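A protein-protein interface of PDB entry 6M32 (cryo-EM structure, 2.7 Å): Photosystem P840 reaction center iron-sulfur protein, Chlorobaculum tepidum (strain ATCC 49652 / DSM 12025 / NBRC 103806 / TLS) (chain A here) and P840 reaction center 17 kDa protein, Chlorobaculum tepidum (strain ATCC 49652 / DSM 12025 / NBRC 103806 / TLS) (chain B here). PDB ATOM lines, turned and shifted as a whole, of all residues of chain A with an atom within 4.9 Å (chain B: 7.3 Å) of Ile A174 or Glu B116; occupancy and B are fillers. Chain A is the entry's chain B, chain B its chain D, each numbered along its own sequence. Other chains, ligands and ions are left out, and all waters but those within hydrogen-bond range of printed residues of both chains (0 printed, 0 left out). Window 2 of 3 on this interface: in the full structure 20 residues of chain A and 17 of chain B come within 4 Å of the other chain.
N of Met B114 lies within hydrogen-bond range of OG1 of Thr B81.
Of the 11 printed residues of chain A, 4 touch a printed residue of chain B.
Hydrophobic or aromatic side chains of chain B that line the printed part of chain A: Met B114.
Among the printed residues, 4 pairs touch across the chains.
Of the printed residues of chain B, Ile A174 touches Glu B116.
Glu B116 touches just these residues of chain A: Tyr A173 (3.6 Å) and Ile A174 (3.8 Å).
Printed residues of chain B within 4 Å of Tyr A173: Glu B116 (3.6 Å).
Printed residues of chain B within 4 Å of Phe A134: Met B114 (3.9 Å).
Of the printed residues of chain B, Ile A135 touches Met B114.
Of the printed residues of chain A, Met B114 touches Phe A134 (3.9 Å) and Ile A135 (3.8 Å).
The nearest residue of chain B that does not touch Ile A174 is Met B114 (6.5 Å).
The nearest printed residue of chain A that does not touch Met B114 is Tyr A133 (6.4 Å).
Among the printed residues, merely in contact across the chains: Phe A134 with Met B114, Ile A135 with Met B114, Tyr A173 with Glu B116 and Ile A174 with Glu B116.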
ATOM      1  N   TYR A 133      -4.135   5.521  -8.484  1.00  0.00           N
ATOM      2  CA  TYR A 133      -3.251   4.392  -8.780  1.00  0.00           C
ATOM      3  C   TYR A 133      -2.320   4.584  -9.973  1.00  0.00           C
ATOM      4  O   TYR A 133      -1.169   4.151  -9.900  1.00  0.00           O
ATOM      5  CB  TYR A 133      -4.093   3.125  -8.952  1.00  0.00           C
ATOM      6  CG  TYR A 133      -4.695   2.699  -7.635  1.00  0.00           C
ATOM      7  CD1 TYR A 133      -4.039   1.803  -6.803  1.00  0.00           C
ATOM      8  CD2 TYR A 133      -5.899   3.230  -7.202  1.00  0.00           C
ATOM      9  CE1 TYR A 133      -4.585   1.428  -5.593  1.00  0.00           C
ATOM     10  CE2 TYR A 133      -6.446   2.862  -5.996  1.00  0.00           C
ATOM     11  CZ  TYR A 133      -5.785   1.967  -5.194  1.00  0.00           C
ATOM     12  OH  TYR A 133      -6.341   1.610  -3.991  1.00  0.00           O
ATOM     13  N   PHE A 134      -2.772   5.177 -11.083  1.00  0.00           N
ATOM     14  CA  PHE A 134      -1.881   5.838 -12.047  1.00  0.00           C
ATOM     15  C   PHE A 134      -0.816   4.897 -12.629  1.00  0.00           C
ATOM     16  O   PHE A 134       0.360   4.964 -12.276  1.00  0.00           O
ATOM     17  CB  PHE A 134      -1.202   7.052 -11.404  1.00  0.00           C
ATOM     18  CG  PHE A 134      -2.094   8.239 -11.264  1.00  0.00           C
ATOM     19  CD1 PHE A 134      -2.877   8.660 -12.319  1.00  0.00           C
ATOM     20  CD2 PHE A 134      -2.148   8.938 -10.074  1.00  0.00           C
ATOM     21  CE1 PHE A 134      -3.699   9.756 -12.191  1.00  0.00           C
ATOM     22  CE2 PHE A 134      -2.968  10.036  -9.940  1.00  0.00           C
ATOM     23  CZ  PHE A 134      -3.745  10.444 -10.998  1.00  0.00           C
ATOM     24  N   ILE A 135      -1.257   3.987 -13.503  1.00  0.00           N
ATOM     25  CA  ILE A 135      -0.304   3.217 -14.303  1.00  0.00           C
ATOM     26  C   ILE A 135       0.693   4.152 -14.979  1.00  0.00           C
ATOM     27  O   ILE A 135       0.308   5.156 -15.587  1.00  0.00           O
ATOM     28  CB  ILE A 135      -1.037   2.360 -15.353  1.00  0.00           C
ATOM     29  CG1 ILE A 135      -1.716   1.155 -14.711  1.00  0.00           C
ATOM     30  CG2 ILE A 135      -0.079   1.897 -16.434  1.00  0.00           C
ATOM     31  CD1 ILE A 135      -2.478   0.306 -15.699  1.00  0.00           C
ATOM     32  N   ALA A 156     -12.187   0.401 -15.846  1.00  0.00           N
ATOM     33  CA  ALA A 156     -11.305   1.549 -15.687  1.00  0.00           C
ATOM     34  C   ALA A 156      -9.965   1.369 -16.382  1.00  0.00           C
ATOM     35  O   ALA A 156      -9.242   2.354 -16.560  1.00  0.00           O
ATOM     36  CB  ALA A 156     -11.075   1.831 -14.203  1.00  0.00           C
ATOM     37  N   ILE A 157      -9.621   0.151 -16.783  1.00  0.00           N
ATOM     38  CA  ILE A 157      -8.327  -0.149 -17.381  1.00  0.00           C
ATOM     39  C   ILE A 157      -8.531  -0.509 -18.844  1.00  0.00           C
ATOM     40  O   ILE A 157      -9.431  -1.286 -19.184  1.00  0.00           O
ATOM     41  CB  ILE A 157      -7.611  -1.284 -16.626  1.00  0.00           C
ATOM     42  CG1 ILE A 157      -7.505  -0.938 -15.145  1.00  0.00           C
ATOM     43  CG2 ILE A 157      -6.236  -1.524 -17.208  1.00  0.00           C
ATOM     44  CD1 ILE A 157      -6.642  -1.888 -14.366  1.00  0.00           C
ATOM     45  N   CYS A 172      -0.909  -0.463 -21.595  1.00  0.00           N
ATOM     46  CA  CYS A 172      -2.243  -0.231 -21.068  1.00  0.00           C
ATOM     47  C   CYS A 172      -2.290   1.078 -20.283  1.00  0.00           C
ATOM     48  O   CYS A 172      -1.290   1.782 -20.133  1.00  0.00           O
ATOM     49  CB  CYS A 172      -2.681  -1.401 -20.192  1.00  0.00           C
ATOM     50  SG  CYS A 172      -1.706  -1.586 -18.694  1.00  0.00           S
ATOM     51  N   TYR A 173      -3.469   1.407 -19.767  1.00  0.00           N
ATOM     52  CA  TYR A 173      -3.666   2.657 -19.042  1.00  0.00           C
ATOM     53  C   TYR A 173      -4.889   2.520 -18.143  1.00  0.00           C
ATOM     54  O   TYR A 173      -5.662   1.563 -18.258  1.00  0.00           O
ATOM     55  CB  TYR A 173      -3.820   3.831 -20.012  1.00  0.00           C
ATOM     56  CG  TYR A 173      -5.159   3.855 -20.699  1.00  0.00           C
ATOM     57  CD1 TYR A 173      -5.415   3.033 -21.784  1.00  0.00           C
ATOM     58  CD2 TYR A 173      -6.171   4.691 -20.257  1.00  0.00           C
ATOM     59  CE1 TYR A 173      -6.640   3.049 -22.416  1.00  0.00           C
ATOM     60  CE2 TYR A 173      -7.399   4.714 -20.882  1.00  0.00           C
ATOM     61  CZ  TYR A 173      -7.628   3.889 -21.961  1.00  0.00           C
ATOM     62  OH  TYR A 173      -8.849   3.905 -22.590  1.00  0.00           O
ATOM     63  N   ILE A 174      -5.082   3.504 -17.265  1.00  0.00           N
ATOM     64  CA  ILE A 174      -6.175   3.517 -16.298  1.00  0.00           C
ATOM     65  C   ILE A 174      -7.034   4.747 -16.549  1.00  0.00           C
ATOM     66  O   ILE A 174      -6.512   5.860 -16.664  1.00  0.00           O
ATOM     67  CB  ILE A 174      -5.659   3.524 -14.846  1.00  0.00           C
ATOM     68  CG1 ILE A 174      -5.230   2.124 -14.420  1.00  0.00           C
ATOM     69  CG2 ILE A 174      -6.718   4.057 -13.897  1.00  0.00           C
ATOM     70  CD1 ILE A 174      -4.830   2.034 -12.972  1.00  0.00           C
ATOM     71  N   ASP A 175      -8.347   4.551 -16.628  1.00  0.00           N
ATOM     72  CA  ASP A 175      -9.278   5.665 -16.744  1.00  0.00           C
ATOM     73  C   ASP A 175      -9.647   6.159 -15.351  1.00  0.00           C
ATOM     74  O   ASP A 175     -10.152   5.391 -14.527  1.00  0.00           O
ATOM     75  CB  ASP A 175     -10.523   5.244 -17.516  1.00  0.00           C
ATOM     76  CG  ASP A 175     -11.580   6.328 -17.550  1.00  0.00           C
ATOM     77  OD1 ASP A 175     -11.251   7.466 -17.939  1.00  0.00           O
ATOM     78  OD2 ASP A 175     -12.739   6.041 -17.189  1.00  0.00           O
ATOM     79  N   GLN A 176      -9.398   7.442 -15.088  1.00  0.00           N
ATOM     80  CA  GLN A 176      -9.611   7.987 -13.754  1.00  0.00           C
ATOM     81  C   GLN A 176     -11.065   8.340 -13.478  1.00  0.00           C
ATOM     82  O   GLN A 176     -11.432   8.520 -12.313  1.00  0.00           O
ATOM     83  CB  GLN A 176      -8.739   9.226 -13.550  1.00  0.00           C
ATOM     84  CG  GLN A 176      -7.250   8.943 -13.606  1.00  0.00           C
ATOM     85  CD  GLN A 176      -6.795   8.008 -12.507  1.00  0.00           C
ATOM     86  OE1 GLN A 176      -7.412   7.929 -11.448  1.00  0.00           O
ATOM     87  NE2 GLN A 176      -5.710   7.290 -12.758  1.00  0.00           N
ATOM     88  N   CYS A 179     -12.470   4.585 -12.273  1.00  0.00           N
ATOM     89  CA  CYS A 179     -11.814   3.909 -11.164  1.00  0.00           C
ATOM     90  C   CYS A 179     -12.479   4.275  -9.843  1.00  0.00           C
ATOM     91  O   CYS A 179     -12.854   5.426  -9.607  1.00  0.00           O
ATOM     92  CB  CYS A 179     -10.332   4.279 -11.124  1.00  0.00           C
ATOM     93  SG  CYS A 179      -9.417   3.565  -9.751  1.00  0.00           S
ATOM     94  N   THR B  81       4.171  13.481 -14.608  1.00  0.00           N
ATOM     95  CA  THR B  81       3.401  14.487 -15.353  1.00  0.00           C
ATOM     96  C   THR B  81       2.080  14.917 -14.711  1.00  0.00           C
ATOM     97  O   THR B  81       1.485  15.911 -15.137  1.00  0.00           O
ATOM     98  CB  THR B  81       3.082  13.997 -16.769  1.00  0.00           C
ATOM     99  OG1 THR B  81       2.149  12.911 -16.706  1.00  0.00           O
ATOM    100  CG2 THR B  81       4.324  13.558 -17.484  1.00  0.00           C
ATOM    101  N   THR B 113       5.878   9.595 -17.873  1.00  0.00           N
ATOM    102  CA  THR B 113       4.630  10.104 -18.425  1.00  0.00           C
ATOM    103  C   THR B 113       3.484   9.168 -18.067  1.00  0.00           C
ATOM    104  O   THR B 113       3.673   7.953 -17.964  1.00  0.00           O
ATOM    105  CB  THR B 113       4.722  10.269 -19.944  1.00  0.00           C
ATOM    106  OG1 THR B 113       4.985   9.000 -20.550  1.00  0.00           O
ATOM    107  CG2 THR B 113       5.839  11.234 -20.304  1.00  0.00           C
ATOM    108  N   MET B 114       2.298   9.740 -17.852  1.00  0.00           N
ATOM    109  CA  MET B 114       1.138   8.978 -17.399  1.00  0.00           C
ATOM    110  C   MET B 114      -0.121   9.439 -18.110  1.00  0.00           C
ATOM    111  O   MET B 114      -1.206   9.477 -17.520  1.00  0.00           O
ATOM    112  CB  MET B 114       0.955   9.113 -15.893  1.00  0.00           C
ATOM    113  CG  MET B 114       2.055   8.475 -15.112  1.00  0.00           C
ATOM    114  SD  MET B 114       1.832   8.652 -13.351  1.00  0.00           S
ATOM    115  CE  MET B 114       3.349   7.884 -12.829  1.00  0.00           C
ATOM    116  N   ARG B 115      -0.001   9.796 -19.382  1.00  0.00           N
ATOM    117  CA  ARG B 115      -1.103  10.435 -20.087  1.00  0.00           C
ATOM    118  C   ARG B 115      -2.273   9.468 -20.227  1.00  0.00           C
ATOM    119  O   ARG B 115      -2.186   8.474 -20.954  1.00  0.00           O
ATOM    120  CB  ARG B 115      -0.627  10.928 -21.450  1.00  0.00           C
ATOM    121  CG  ARG B 115       0.679  11.704 -21.371  1.00  0.00           C
ATOM    122  CD  ARG B 115       0.769  12.794 -22.424  1.00  0.00           C
ATOM    123  NE  ARG B 115       1.917  13.667 -22.190  1.00  0.00           N
ATOM    124  CZ  ARG B 115       2.124  14.819 -22.819  1.00  0.00           C
ATOM    125  NH1 ARG B 115       1.257  15.247 -23.727  1.00  0.00           N
ATOM    126  NH2 ARG B 115       3.198  15.545 -22.540  1.00  0.00           N
ATOM    127  N   GLU B 116      -3.366   9.761 -19.516  1.00  0.00           N
ATOM    128  CA  GLU B 116      -4.536   8.890 -19.531  1.00  0.00           C
ATOM    129  C   GLU B 116      -5.373   9.088 -20.789  1.00  0.00           C
ATOM    130  O   GLU B 116      -6.123   8.189 -21.183  1.00  0.00           O
ATOM    131  CB  GLU B 116      -5.388   9.128 -18.284  1.00  0.00           C
ATOM    132  CG  GLU B 116      -5.851  10.564 -18.098  1.00  0.00           C
ATOM    133  CD  GLU B 116      -7.216  10.820 -18.705  1.00  0.00           C
ATOM    134  OE1 GLU B 116      -7.912   9.841 -19.044  1.00  0.00           O
ATOM    135  OE2 GLU B 116      -7.597  12.002 -18.834  1.00  0.00           O
ATOM    136  N   ILE B 117      -5.272  10.252 -21.420  1.00  0.00           N
ATOM    137  CA  ILE B 117      -5.997  10.501 -22.658  1.00  0.00           C
ATOM    138  C   ILE B 117      -5.253   9.873 -23.831  1.00  0.00           C
ATOM    139  O   ILE B 117      -5.786   9.009 -24.525  1.00  0.00           O
ATOM    140  CB  ILE B 117      -6.211  12.003 -22.890  1.00  0.00           C
ATOM    141  CG1 ILE B 117      -7.228  12.557 -21.892  1.00  0.00           C
ATOM    142  CG2 ILE B 117      -6.663  12.261 -24.320  1.00  0.00           C
ATOM    143  CD1 ILE B 117      -8.650  12.098 -22.145  1.00  0.00           C
